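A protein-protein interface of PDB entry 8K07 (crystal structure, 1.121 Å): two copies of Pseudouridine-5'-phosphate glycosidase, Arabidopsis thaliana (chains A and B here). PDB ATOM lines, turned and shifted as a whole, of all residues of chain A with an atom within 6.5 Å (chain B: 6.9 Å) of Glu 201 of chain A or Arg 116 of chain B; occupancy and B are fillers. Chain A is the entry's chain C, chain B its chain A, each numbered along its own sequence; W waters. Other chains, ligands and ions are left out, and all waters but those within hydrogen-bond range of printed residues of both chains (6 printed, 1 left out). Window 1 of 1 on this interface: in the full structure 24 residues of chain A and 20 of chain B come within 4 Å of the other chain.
Position printed for both chains: 172.
Of the 20 pairs that touch across the chains among the printed residues, none has its exchanged pair printed and touching as well.
ND2 of Asn 241 of chain A sits at hydrogen-bond distance from O of Ala 248 of chain A (3.0 Å).
The backbone carbonyl oxygen (O) of Asn 241 of chain A lies within hydrogen-bond range of the backbone NH (N) of Arg 246 of chain A (3.3 Å).
The backbone carbonyl oxygen (O) of Glu 195 of chain A lies within hydrogen-bond range of the side-chain hydroxyl (OG1) of Thr 199 of chain A (3.1 Å).
Among the printed residues, pairs that only touch across the chains: Glu 198 of chain A with Ser 167 of chain B (3.4 Å), Thr 199 of chain A with Ser 167 of chain B (3.8 Å), Glu 201 of chain A with Gly 115 of chain B (3.4 Å), Glu 201 of chain A with Arg 116 of chain B (3.4 Å), Glu 201 of chain A with Ser 167 of chain B (3.9 Å), Glu 201 of chain A with Ala 171 of chain B (3.4 Å), Tyr 203 of chain A with Arg 116 of chain B (3.2 Å), Val 204 of chain A with Arg 116 of chain B (3.9 Å), Pro 225 of chain A with Arg 116 of chain B (3.5 Å), Asn 241 of chain A with Ala 119 of chain B (3.8 Å), Arg 246 of chain A with Arg 116 of chain B (3.9 Å) and Arg 246 of chain A with Phe 137 of chain B (3.4 Å).
Of the printed residues of chain B, Gly 173 of chain A touches Arg 174.
Printed residues of chain B within 4 Å of Gln 200 of chain A: Arg 174.
Glu 201 of chain A touches just these residues of chain B: Gly 115, Arg 116, Ser 167 and Ala 171.
Arg 116 of chain B touches just these residues of chain A: Glu 198 (3.5 Å), Glu 201 (3.4 Å), Val 202 (3.0 Å), Tyr 203 (3.2 Å), Val 204 (3.9 Å), Pro 225 (3.5 Å) and Arg 246 (3.9 Å).
Printed residues of chain A within 4 Å of Thr 170 of chain B: Thr 199 (2.8 Å).
The nearest residue of chain B that does not touch Glu 201 of chain A is Ser 133 of chain B (4.1 Å).
The nearest residue of chain A that does not touch Arg 116 of chain B is Leu 197 of chain A (4.4 Å).
The nearest printed residue of chain A that does not touch Ser 167 of chain B is Gln 200 of chain A (5.3 Å).
Water W2 bridges OE1 of Gln 200 of chain A (2.7 Å) and NH1 of Arg 174 of chain B (3.0 Å).
Water W4 lies within hydrogen-bond range of the backbone carbonyl oxygen of Ser 133 of chain B (2.9 Å), the side-chain carboxylate of Glu 201 of chain A (2.9 Å) and the guanidinium group of Arg 246 of chain A (3.1 Å).
Of the 19 printed residues of chain A, 12 touch a printed residue of chain B.
Hydrophobic or aromatic side chains of chain B within 4 Å of the printed part of chain A: Ala 119, Phe 137 and Ala 171.
The side-chain amide oxygen of Asn 120 of chain B lies close to the side-chain hydroxyl of Tyr 203 of chain A (3.4 Å).
The side-chain carboxylate of Glu 198 of chain A is in salt-bridge range of the guanidinium group of Arg 116 of chain B.
The guanidinium group (NH1) of Arg 116 of chain B is in hydrogen-bond range of the backbone carbonyl oxygen (O) of Val 202 of chain A.
The backbone carbonyl oxygen (O) of Gly 173 of chain A is in hydrogen-bond range of the guanidinium group (NH2) of Arg 174 of chain B, at 3.2 Å.
The backbone carbonyl oxygen of Gly 115 of chain B sits close to the guanidinium group of Arg 246 of chain A, at 3.4 Å.
O of Gln 200 of chain A lies within hydrogen-bond range of NH2 of Arg 174 of chain B, at 3.0 Å.
OG1 of Thr 170 of chain B is in hydrogen-bond range of O of Thr 199 of chain A (2.8 Å).
The side-chain amide nitrogen (ND2) of Asn 120 of chain B is in hydrogen-bond range of the side-chain hydroxyl (OG) of Ser 226 of chain A, 3.4 Å away.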
ATOM      1  N   LEU A 172     -21.394  -1.644   8.270  1.00  0.00           N
ATOM      2  CA  LEU A 172     -21.470  -3.083   8.120  1.00  0.00           C
ATOM      3  C   LEU A 172     -20.885  -3.784   9.356  1.00  0.00           C
ATOM      4  O   LEU A 172     -21.342  -4.865   9.726  1.00  0.00           O
ATOM      5  CB  LEU A 172     -20.766  -3.530   6.838  1.00  0.00           C
ATOM      6  CG  LEU A 172     -20.972  -4.987   6.432  1.00  0.00           C
ATOM      7  CD1 LEU A 172     -22.440  -5.372   6.474  1.00  0.00           C
ATOM      8  CD2 LEU A 172     -20.394  -5.204   5.042  1.00  0.00           C
ATOM      9  N   GLY A 173     -19.898  -3.162  10.001  1.00  0.00           N
ATOM     10  CA  GLY A 173     -19.315  -3.701  11.216  1.00  0.00           C
ATOM     11  C   GLY A 173     -20.247  -3.703  12.415  1.00  0.00           C
ATOM     12  O   GLY A 173     -19.944  -4.341  13.425  1.00  0.00           O
ATOM     13  N   LEU A 194      -9.913  -3.871   2.771  1.00  0.00           N
ATOM     14  CA  LEU A 194      -9.934  -5.187   3.397  1.00  0.00           C
ATOM     15  C   LEU A 194      -9.443  -5.116   4.851  1.00  0.00           C
ATOM     16  O   LEU A 194     -10.036  -5.747   5.726  1.00  0.00           O
ATOM     17  CB  LEU A 194      -9.091  -6.175   2.589  1.00  0.00           C
ATOM     18  CG  LEU A 194      -9.709  -6.577   1.247  1.00  0.00           C
ATOM     19  CD1 LEU A 194      -8.723  -7.399   0.432  1.00  0.00           C
ATOM     20  CD2 LEU A 194     -11.005  -7.348   1.453  1.00  0.00           C
ATOM     21  N   GLU A 195      -8.384  -4.348   5.117  1.00  0.00           N
ATOM     22  CA  GLU A 195      -7.912  -4.205   6.491  1.00  0.00           C
ATOM     23  C   GLU A 195      -8.964  -3.550   7.384  1.00  0.00           C
ATOM     24  O   GLU A 195      -9.199  -4.010   8.500  1.00  0.00           O
ATOM     25  CB  GLU A 195      -6.618  -3.393   6.546  1.00  0.00           C
ATOM     26  CG  GLU A 195      -5.400  -4.062   5.924  1.00  0.00           C
ATOM     27  CD  GLU A 195      -4.952  -5.322   6.650  1.00  0.00           C
ATOM     28  OE1 GLU A 195      -5.292  -5.523   7.840  1.00  0.00           O
ATOM     29  OE2 GLU A 195      -4.238  -6.130   6.020  1.00  0.00           O
ATOM     30  N   TYR A 196      -9.593  -2.485   6.898  1.00  0.00           N
ATOM     31  CA  TYR A 196     -10.568  -1.755   7.704  1.00  0.00           C
ATOM     32  C   TYR A 196     -11.780  -2.636   7.996  1.00  0.00           C
ATOM     33  O   TYR A 196     -12.258  -2.677   9.139  1.00  0.00           O
ATOM     34  CB  TYR A 196     -10.982  -0.439   7.025  1.00  0.00           C
ATOM     35  CG  TYR A 196     -11.816   0.433   7.938  1.00  0.00           C
ATOM     36  CD1 TYR A 196     -11.244   1.247   8.900  1.00  0.00           C
ATOM     37  CD2 TYR A 196     -13.193   0.396   7.868  1.00  0.00           C
ATOM     38  CE1 TYR A 196     -12.045   2.025   9.740  1.00  0.00           C
ATOM     39  CE2 TYR A 196     -13.991   1.165   8.686  1.00  0.00           C
ATOM     40  CZ  TYR A 196     -13.421   1.964   9.622  1.00  0.00           C
ATOM     41  OH  TYR A 196     -14.235   2.717  10.449  1.00  0.00           O
ATOM     42  N   LEU A 197     -12.238  -3.386   7.002  1.00  0.00           N
ATOM     43  CA  LEU A 197     -13.304  -4.349   7.231  1.00  0.00           C
ATOM     44  C   LEU A 197     -12.940  -5.348   8.317  1.00  0.00           C
ATOM     45  O   LEU A 197     -13.779  -5.673   9.169  1.00  0.00           O
ATOM     46  CB  LEU A 197     -13.646  -5.084   5.936  1.00  0.00           C
ATOM     47  CG  LEU A 197     -14.470  -4.253   4.943  1.00  0.00           C
ATOM     48  CD1 LEU A 197     -14.425  -4.859   3.546  1.00  0.00           C
ATOM     49  CD2 LEU A 197     -15.899  -4.135   5.422  1.00  0.00           C
ATOM     50  N   GLU A 198     -11.708  -5.849   8.284  1.00  0.00           N
ATOM     51  CA  GLU A 198     -11.265  -6.777   9.309  1.00  0.00           C
ATOM     52  C   GLU A 198     -11.285  -6.110  10.693  1.00  0.00           C
ATOM     53  O   GLU A 198     -11.758  -6.704  11.655  1.00  0.00           O
ATOM     54  CB  GLU A 198      -9.873  -7.326   8.988  1.00  0.00           C
ATOM     55  CG  GLU A 198      -9.469  -8.383   9.995  1.00  0.00           C
ATOM     56  CD  GLU A 198      -8.199  -9.131   9.651  1.00  0.00           C
ATOM     57  OE1 GLU A 198      -7.498  -8.769   8.690  1.00  0.00           O
ATOM     58  OE2 GLU A 198      -7.903 -10.111  10.366  1.00  0.00           O
ATOM     59  N   THR A 199     -10.799  -4.883  10.784  1.00  0.00           N
ATOM     60  CA  THR A 199     -10.795  -4.154  12.051  1.00  0.00           C
ATOM     61  C   THR A 199     -12.214  -3.974  12.588  1.00  0.00           C
ATOM     62  O   THR A 199     -12.432  -3.995  13.813  1.00  0.00           O
ATOM     63  CB  THR A 199     -10.098  -2.801  11.874  1.00  0.00           C
ATOM     64  OG1 THR A 199      -8.781  -3.029  11.358  1.00  0.00           O
ATOM     65  CG2 THR A 199      -9.996  -2.041  13.189  1.00  0.00           C
ATOM     66  N   GLN A 200     -13.176  -3.811  11.678  1.00  0.00           N
ATOM     67  CA  GLN A 200     -14.566  -3.628  12.068  1.00  0.00           C
ATOM     68  C   GLN A 200     -15.325  -4.925  12.328  1.00  0.00           C
ATOM     69  O   GLN A 200     -16.536  -4.885  12.549  1.00  0.00           O
ATOM     70  CB  GLN A 200     -15.309  -2.822  10.998  1.00  0.00           C
ATOM     71  CG  GLN A 200     -14.707  -1.456  10.725  1.00  0.00           C
ATOM     72  CD  GLN A 200     -14.642  -0.569  11.960  1.00  0.00           C
ATOM     73  OE1 GLN A 200     -15.645  -0.343  12.633  1.00  0.00           O
ATOM     74  NE2 GLN A 200     -13.448  -0.076  12.271  1.00  0.00           N
ATOM     75  N   GLU A 201     -14.628  -6.062  12.279  1.00  0.00           N
ATOM     76  CA  GLU A 201     -15.192  -7.398  12.533  1.00  0.00           C
ATOM     77  C   GLU A 201     -16.150  -7.925  11.470  1.00  0.00           C
ATOM     78  O   GLU A 201     -16.985  -8.790  11.750  1.00  0.00           O
ATOM     79  CB  GLU A 201     -15.899  -7.482  13.893  1.00  0.00           C
ATOM     80  CG  GLU A 201     -14.970  -7.438  15.086  1.00  0.00           C
ATOM     81  CD  GLU A 201     -15.440  -8.368  16.211  1.00  0.00           C
ATOM     82  OE1 GLU A 201     -15.412  -9.638  16.057  1.00  0.00           O
ATOM     83  OE2 GLU A 201     -15.875  -7.783  17.232  1.00  0.00           O
ATOM     84  N   VAL A 202     -15.979  -7.461  10.237  1.00  0.00           N
ATOM     85  CA  VAL A 202     -16.805  -7.914   9.121  1.00  0.00           C
ATOM     86  C   VAL A 202     -16.214  -9.139   8.446  1.00  0.00           C
ATOM     87  O   VAL A 202     -15.091  -9.084   7.968  1.00  0.00           O
ATOM     88  CB  VAL A 202     -16.980  -6.795   8.086  1.00  0.00           C
ATOM     89  CG1 VAL A 202     -17.753  -7.295   6.896  1.00  0.00           C
ATOM     90  CG2 VAL A 202     -17.671  -5.591   8.724  1.00  0.00           C
ATOM     91  N   TYR A 203     -16.970 -10.235   8.421  1.00  0.00           N
ATOM     92  CA  TYR A 203     -16.594 -11.421   7.669  1.00  0.00           C
ATOM     93  C   TYR A 203     -16.660 -11.123   6.184  1.00  0.00           C
ATOM     94  O   TYR A 203     -17.694 -10.673   5.681  1.00  0.00           O
ATOM     95  CB  TYR A 203     -17.507 -12.590   8.018  1.00  0.00           C
ATOM     96  CG  TYR A 203     -17.201 -13.835   7.240  1.00  0.00           C
ATOM     97  CD1 TYR A 203     -15.993 -14.488   7.390  1.00  0.00           C
ATOM     98  CD2 TYR A 203     -18.115 -14.347   6.331  1.00  0.00           C
ATOM     99  CE1 TYR A 203     -15.715 -15.635   6.665  1.00  0.00           C
ATOM    100  CE2 TYR A 203     -17.856 -15.482   5.613  1.00  0.00           C
ATOM    101  CZ  TYR A 203     -16.656 -16.124   5.771  1.00  0.00           C
ATOM    102  OH  TYR A 203     -16.429 -17.264   5.019  1.00  0.00           O
ATOM    103  N   VAL A 204     -15.543 -11.346   5.501  1.00  0.00           N
ATOM    104  CA  VAL A 204     -15.422 -11.118   4.070  1.00  0.00           C
ATOM    105  C   VAL A 204     -15.108 -12.441   3.367  1.00  0.00           C
ATOM    106  O   VAL A 204     -14.143 -13.130   3.723  1.00  0.00           O
ATOM    107  CB  VAL A 204     -14.320 -10.094   3.761  1.00  0.00           C
ATOM    108  CG1 VAL A 204     -14.180  -9.896   2.262  1.00  0.00           C
ATOM    109  CG2 VAL A 204     -14.612  -8.765   4.441  1.00  0.00           C
ATOM    110  N   PRO A 225      -9.841 -13.223   2.146  1.00  0.00           N
ATOM    111  CA  PRO A 225      -9.557 -13.781   3.474  1.00  0.00           C
ATOM    112  C   PRO A 225     -10.344 -15.056   3.758  1.00  0.00           C
ATOM    113  O   PRO A 225      -9.973 -15.810   4.652  1.00  0.00           O
ATOM    114  CB  PRO A 225      -9.962 -12.653   4.428  1.00  0.00           C
ATOM    115  CG  PRO A 225     -10.961 -11.869   3.672  1.00  0.00           C
ATOM    116  CD  PRO A 225     -10.530 -11.923   2.230  1.00  0.00           C
ATOM    117  N   SER A 226     -11.424 -15.284   3.015  1.00  0.00           N
ATOM    118  CA  SER A 226     -12.218 -16.497   3.162  1.00  0.00           C
ATOM    119  C   SER A 226     -12.964 -16.745   1.860  1.00  0.00           C
ATOM    120  O   SER A 226     -13.011 -15.868   0.999  1.00  0.00           O
ATOM    121  CB  SER A 226     -13.192 -16.388   4.344  1.00  0.00           C
ATOM    122  OG  SER A 226     -13.793 -17.645   4.628  1.00  0.00           O
ATOM    123  N   ASN A 241     -24.620 -16.682  11.860  1.00  0.00           N
ATOM    124  CA  ASN A 241     -24.440 -15.318  12.338  1.00  0.00           C
ATOM    125  C   ASN A 241     -25.691 -14.821  13.045  1.00  0.00           C
ATOM    126  O   ASN A 241     -25.610 -14.157  14.084  1.00  0.00           O
ATOM    127  CB  ASN A 241     -24.093 -14.394  11.170  1.00  0.00           C
ATOM    128  CG  ASN A 241     -23.286 -13.191  11.598  1.00  0.00           C
ATOM    129  OD1 ASN A 241     -22.213 -13.344  12.181  1.00  0.00           O
ATOM    130  ND2 ASN A 241     -23.776 -11.991  11.300  1.00  0.00           N
ATOM    131  N   ARG A 246     -24.647 -12.213  16.564  1.00  0.00           N
ATOM    132  CA  ARG A 246     -23.552 -11.275  16.315  1.00  0.00           C
ATOM    133  C   ARG A 246     -24.079  -9.973  15.746  1.00  0.00           C
ATOM    134  O   ARG A 246     -25.071  -9.952  15.019  1.00  0.00           O
ATOM    135  CB  ARG A 246     -22.484 -11.878  15.398  1.00  0.00           C
ATOM    136  CG  ARG A 246     -21.686 -12.932  16.140  1.00  0.00           C
ATOM    137  CD  ARG A 246     -20.295 -13.255  15.609  1.00  0.00           C
ATOM    138  NE  ARG A 246     -19.431 -12.143  15.199  1.00  0.00           N
ATOM    139  CZ  ARG A 246     -18.521 -11.479  15.917  1.00  0.00           C
ATOM    140  NH1 ARG A 246     -18.304 -11.689  17.216  1.00  0.00           N
ATOM    141  NH2 ARG A 246     -17.817 -10.550  15.294  1.00  0.00           N
ATOM    142  N   ALA A 248     -22.157  -7.740  13.966  1.00  0.00           N
ATOM    143  CA  ALA A 248     -21.443  -7.376  12.760  1.00  0.00           C
ATOM    144  C   ALA A 248     -21.974  -8.164  11.578  1.00  0.00           C
ATOM    145  O   ALA A 248     -22.417  -9.310  11.712  1.00  0.00           O
ATOM    146  CB  ALA A 248     -19.948  -7.613  12.921  1.00  0.00           C
ATOM    147  N   GLY A 249     -21.911  -7.542  10.413  1.00  0.00           N
ATOM    148  CA  GLY A 249     -22.422  -8.137   9.202  1.00  0.00           C
ATOM    149  C   GLY A 249     -21.362  -8.820   8.370  1.00  0.00           C
ATOM    150  O   GLY A 249     -20.243  -9.104   8.811  1.00  0.00           O
ATOM    151  N   THR B 113      -9.291 -18.388  14.717  1.00  0.00           N
ATOM    152  CA  THR B 113     -10.656 -17.906  14.577  1.00  0.00           C
ATOM    153  C   THR B 113     -10.854 -16.581  15.293  1.00  0.00           C
ATOM    154  O   THR B 113     -10.927 -16.535  16.529  1.00  0.00           O
ATOM    155  CB  THR B 113     -11.629 -18.952  15.131  1.00  0.00           C
ATOM    156  OG1 THR B 113     -11.439 -20.176  14.421  1.00  0.00           O
ATOM    157  CG2 THR B 113     -13.077 -18.523  14.965  1.00  0.00           C
ATOM    158  N   ALA B 114     -10.913 -15.495  14.525  1.00  0.00           N
ATOM    159  CA  ALA B 114     -11.285 -14.199  15.077  1.00  0.00           C
ATOM    160  C   ALA B 114     -12.805 -14.144  15.187  1.00  0.00           C
ATOM    161  O   ALA B 114     -13.492 -15.052  14.707  1.00  0.00           O
ATOM    162  CB  ALA B 114     -10.751 -13.064  14.212  1.00  0.00           C
ATOM    163  N   GLY B 115     -13.327 -13.102  15.829  1.00  0.00           N
ATOM    164  CA  GLY B 115     -14.765 -12.969  15.959  1.00  0.00           C
ATOM    165  C   GLY B 115     -15.473 -13.065  14.617  1.00  0.00           C
ATOM    166  O   GLY B 115     -16.521 -13.718  14.522  1.00  0.00           O
ATOM    167  N   ARG B 116     -14.879 -12.472  13.580  1.00  0.00           N
ATOM    168  CA  ARG B 116     -15.526 -12.466  12.276  1.00  0.00           C
ATOM    169  C   ARG B 116     -15.552 -13.834  11.618  1.00  0.00           C
ATOM    170  O   ARG B 116     -16.282 -14.016  10.647  1.00  0.00           O
ATOM    171  CB  ARG B 116     -14.855 -11.465  11.335  1.00  0.00           C
ATOM    172  CG  ARG B 116     -13.514 -11.879  10.784  1.00  0.00           C
ATOM    173  CD  ARG B 116     -13.208 -10.990   9.586  1.00  0.00           C
ATOM    174  NE  ARG B 116     -11.899 -11.225   8.983  1.00  0.00           N
ATOM    175  CZ  ARG B 116     -11.462 -10.556   7.919  1.00  0.00           C
ATOM    176  NH1 ARG B 116     -12.233  -9.621   7.367  1.00  0.00           N
ATOM    177  NH2 ARG B 116     -10.263 -10.807   7.412  1.00  0.00           N
ATOM    178  N   ASP B 117     -14.771 -14.781  12.140  1.00  0.00           N
ATOM    179  CA  ASP B 117     -14.694 -16.124  11.578  1.00  0.00           C
ATOM    180  C   ASP B 117     -15.635 -17.112  12.248  1.00  0.00           C
ATOM    181  O   ASP B 117     -15.796 -18.235  11.767  1.00  0.00           O
ATOM    182  CB  ASP B 117     -13.265 -16.660  11.685  1.00  0.00           C
ATOM    183  CG  ASP B 117     -12.273 -15.815  10.941  1.00  0.00           C
ATOM    184  OD1 ASP B 117     -12.493 -15.628   9.724  1.00  0.00           O
ATOM    185  OD2 ASP B 117     -11.303 -15.341  11.569  1.00  0.00           O
ATOM    186  N   ILE B 118     -16.231 -16.726  13.370  1.00  0.00           N
ATOM    187  CA  ILE B 118     -17.061 -17.647  14.137  1.00  0.00           C
ATOM    188  C   ILE B 118     -18.172 -18.268  13.298  1.00  0.00           C
ATOM    189  O   ILE B 118     -18.323 -19.492  13.255  1.00  0.00           O
ATOM    190  CB  ILE B 118     -17.684 -16.947  15.362  1.00  0.00           C
ATOM    191  CG1 ILE B 118     -16.608 -16.545  16.374  1.00  0.00           C
ATOM    192  CG2 ILE B 118     -18.714 -17.832  16.017  1.00  0.00           C
ATOM    193  CD1 ILE B 118     -17.123 -15.595  17.444  1.00  0.00           C
ATOM    194  N   ALA B 119     -18.945 -17.435  12.612  1.00  0.00           N
ATOM    195  CA  ALA B 119     -20.089 -17.946  11.851  1.00  0.00           C
ATOM    196  C   ALA B 119     -19.652 -18.960  10.795  1.00  0.00           C
ATOM    197  O   ALA B 119     -20.292 -19.993  10.616  1.00  0.00           O
ATOM    198  CB  ALA B 119     -20.863 -16.788  11.216  1.00  0.00           C
ATOM    199  N   ASN B 120     -18.549 -18.677  10.116  1.00  0.00           N
ATOM    200  CA  ASN B 120     -18.028 -19.567   9.088  1.00  0.00           C
ATOM    201  C   ASN B 120     -17.535 -20.892   9.679  1.00  0.00           C
ATOM    202  O   ASN B 120     -17.836 -21.970   9.144  1.00  0.00           O
ATOM    203  CB  ASN B 120     -16.910 -18.875   8.321  1.00  0.00           C
ATOM    204  CG  ASN B 120     -16.421 -19.691   7.161  1.00  0.00           C
ATOM    205  OD1 ASN B 120     -17.214 -20.288   6.427  1.00  0.00           O
ATOM    206  ND2 ASN B 120     -15.107 -19.745   6.988  1.00  0.00           N
ATOM    207  N   VAL B 121     -16.810 -20.836  10.791  1.00  0.00           N
ATOM    208  CA  VAL B 121     -16.318 -22.067  11.401  1.00  0.00           C
ATOM    209  C   VAL B 121     -17.494 -22.902  11.908  1.00  0.00           C
ATOM    210  O   VAL B 121     -17.491 -24.131  11.768  1.00  0.00           O
ATOM    211  CB  VAL B 121     -15.322 -21.781  12.531  1.00  0.00           C
ATOM    212  CG1 VAL B 121     -14.886 -23.083  13.204  1.00  0.00           C
ATOM    213  CG2 VAL B 121     -14.112 -21.061  11.964  1.00  0.00           C
ATOM    214  N   SER B 133     -10.798 -11.396  20.104  1.00  0.00           N
ATOM    215  CA  SER B 133     -12.075 -10.870  19.631  1.00  0.00           C
ATOM    216  C   SER B 133     -13.164 -11.950  19.656  1.00  0.00           C
ATOM    217  O   SER B 133     -14.303 -11.666  20.010  1.00  0.00           O
ATOM    218  CB  SER B 133     -11.936 -10.270  18.224  1.00  0.00           C
ATOM    219  OG  SER B 133     -11.597 -11.250  17.259  1.00  0.00           O
ATOM    220  N   ALA B 134     -12.836 -13.184  19.288  1.00  0.00           N
ATOM    221  CA  ALA B 134     -13.845 -14.247  19.286  1.00  0.00           C
ATOM    222  C   ALA B 134     -14.181 -14.704  20.703  1.00  0.00           C
ATOM    223  O   ALA B 134     -15.337 -14.965  21.027  1.00  0.00           O
ATOM    224  CB  ALA B 134     -13.376 -15.438  18.456  1.00  0.00           C
ATOM    225  N   LEU B 136     -13.944 -12.976  23.488  1.00  0.00           N
ATOM    226  CA  LEU B 136     -14.771 -11.902  24.067  1.00  0.00           C
ATOM    227  C   LEU B 136     -16.246 -12.127  23.804  1.00  0.00           C
ATOM    228  O   LEU B 136     -17.083 -11.965  24.701  1.00  0.00           O
ATOM    229  CB  LEU B 136     -14.388 -10.525  23.487  1.00  0.00           C
ATOM    230  CG  LEU B 136     -13.218  -9.821  24.152  1.00  0.00           C
ATOM    231  CD1 LEU B 136     -12.771  -8.653  23.307  1.00  0.00           C
ATOM    232  CD2 LEU B 136     -13.588  -9.337  25.553  1.00  0.00           C
ATOM    233  N   PHE B 137     -16.562 -12.467  22.555  1.00  0.00           N
ATOM    234  CA  PHE B 137     -17.938 -12.624  22.145  1.00  0.00           C
ATOM    235  C   PHE B 137     -18.597 -13.754  22.936  1.00  0.00           C
ATOM    236  O   PHE B 137     -19.684 -13.587  23.483  1.00  0.00           O
ATOM    237  CB  PHE B 137     -18.032 -12.896  20.648  1.00  0.00           C
ATOM    238  CG  PHE B 137     -19.421 -13.185  20.203  1.00  0.00           C
ATOM    239  CD1 PHE B 137     -20.334 -12.152  20.074  1.00  0.00           C
ATOM    240  CD2 PHE B 137     -19.830 -14.484  19.951  1.00  0.00           C
ATOM    241  CE1 PHE B 137     -21.620 -12.406  19.699  1.00  0.00           C
ATOM    242  CE2 PHE B 137     -21.117 -14.736  19.571  1.00  0.00           C
ATOM    243  CZ  PHE B 137     -22.013 -13.700  19.451  1.00  0.00           C
ATOM    244  N   SER B 167      -8.786  -6.512  15.237  1.00  0.00           N
ATOM    245  CA  SER B 167     -10.179  -6.460  15.669  1.00  0.00           C
ATOM    246  C   SER B 167     -10.328  -6.698  17.173  1.00  0.00           C
ATOM    247  O   SER B 167     -11.382  -6.438  17.727  1.00  0.00           O
ATOM    248  CB  SER B 167     -11.037  -7.471  14.913  1.00  0.00           C
ATOM    249  OG  SER B 167     -10.801  -8.809  15.330  1.00  0.00           O
ATOM    250  N   ASP B 168      -9.295  -7.236  17.813  1.00  0.00           N
ATOM    251  CA  ASP B 168      -9.305  -7.369  19.270  1.00  0.00           C
ATOM    252  C   ASP B 168      -9.646  -6.043  19.941  1.00  0.00           C
ATOM    253  O   ASP B 168     -10.368  -5.995  20.936  1.00  0.00           O
ATOM    254  CB  ASP B 168      -7.946  -7.849  19.786  1.00  0.00           C
ATOM    255  CG  ASP B 168      -7.632  -9.287  19.429  1.00  0.00           C
ATOM    256  OD1 ASP B 168      -8.493 -10.025  18.917  1.00  0.00           O
ATOM    257  OD2 ASP B 168      -6.468  -9.680  19.700  1.00  0.00           O
ATOM    258  N   THR B 170     -11.154  -3.256  18.574  1.00  0.00           N
ATOM    259  CA  THR B 170     -12.505  -2.828  18.273  1.00  0.00           C
ATOM    260  C   THR B 170     -13.499  -3.622  19.121  1.00  0.00           C
ATOM    261  O   THR B 170     -14.435  -3.063  19.707  1.00  0.00           O
ATOM    262  CB  THR B 170     -12.810  -2.993  16.779  1.00  0.00           C
ATOM    263  OG1 THR B 170     -11.742  -2.427  16.008  1.00  0.00           O
ATOM    264  CG2 THR B 170     -14.132  -2.338  16.421  1.00  0.00           C
ATOM    265  N   ALA B 171     -13.287  -4.927  19.205  1.00  0.00           N
ATOM    266  CA  ALA B 171     -14.181  -5.784  19.967  1.00  0.00           C
ATOM    267  C   ALA B 171     -14.218  -5.367  21.442  1.00  0.00           C
ATOM    268  O   ALA B 171     -15.297  -5.298  22.039  1.00  0.00           O
ATOM    269  CB  ALA B 171     -13.759  -7.251  19.838  1.00  0.00           C
ATOM    270  N   LEU B 172     -13.055  -5.089  22.026  1.00  0.00           N
ATOM    271  CA  LEU B 172     -13.008  -4.726  23.434  1.00  0.00           C
ATOM    272  C   LEU B 172     -13.717  -3.393  23.653  1.00  0.00           C
ATOM    273  O   LEU B 172     -14.334  -3.181  24.689  1.00  0.00           O
ATOM    274  CB  LEU B 172     -11.566  -4.688  23.921  1.00  0.00           C
ATOM    275  CG  LEU B 172     -11.399  -4.521  25.424  1.00  0.00           C
ATOM    276  CD1 LEU B 172     -12.272  -5.504  26.178  1.00  0.00           C
ATOM    277  CD2 LEU B 172      -9.937  -4.700  25.772  1.00  0.00           C
ATOM    278  N   ARG B 174     -16.435  -2.483  22.349  1.00  0.00           N
ATOM    279  CA  ARG B 174     -17.891  -2.630  22.370  1.00  0.00           C
ATOM    280  C   ARG B 174     -18.352  -3.948  23.002  1.00  0.00           C
ATOM    281  O   ARG B 174     -19.471  -4.402  22.776  1.00  0.00           O
ATOM    282  CB  ARG B 174     -18.473  -2.424  20.961  1.00  0.00           C
ATOM    283  CG  ARG B 174     -17.873  -3.238  19.852  1.00  0.00           C
ATOM    284  CD  ARG B 174     -18.306  -2.603  18.526  1.00  0.00           C
ATOM    285  NE  ARG B 174     -17.786  -3.281  17.340  1.00  0.00           N
ATOM    286  CZ  ARG B 174     -17.876  -2.801  16.096  1.00  0.00           C
ATOM    287  NH1 ARG B 174     -18.455  -1.630  15.859  1.00  0.00           N
ATOM    288  NH2 ARG B 174     -17.372  -3.497  15.088  1.00  0.00           N
ATOM    289  N   THR B 175     -17.507  -4.517  23.855  1.00  0.00           N
ATOM    290  CA  THR B 175     -17.870  -5.680  24.654  1.00  0.00           C
ATOM    291  C   THR B 175     -17.462  -5.433  26.098  1.00  0.00           C
ATOM    292  O   THR B 175     -16.270  -5.302  26.374  1.00  0.00           O
ATOM    293  CB  THR B 175     -17.176  -6.951  24.167  1.00  0.00           C
ATOM    294  OG1 THR B 175     -17.295  -7.066  22.745  1.00  0.00           O
ATOM    295  CG2 THR B 175     -17.787  -8.171  24.837  1.00  0.00           C
HETATM  296  O   HOH W   1     -11.029  -8.286   5.131  1.00  0.00           O
HETATM  297  O   HOH W   2     -18.245  -1.122  12.936  1.00  0.00           O
HETATM  298  O   HOH W   3     -13.138 -12.677   6.332  1.00  0.00           O
HETATM  299  O   HOH W   4     -16.408  -9.988  19.048  1.00  0.00           O
HETATM  300  O   HOH W   5     -13.176 -10.183  14.459  1.00  0.00           O
HETATM  301  O   HOH W   6     -12.018 -19.004   6.126  1.00  0.00           O
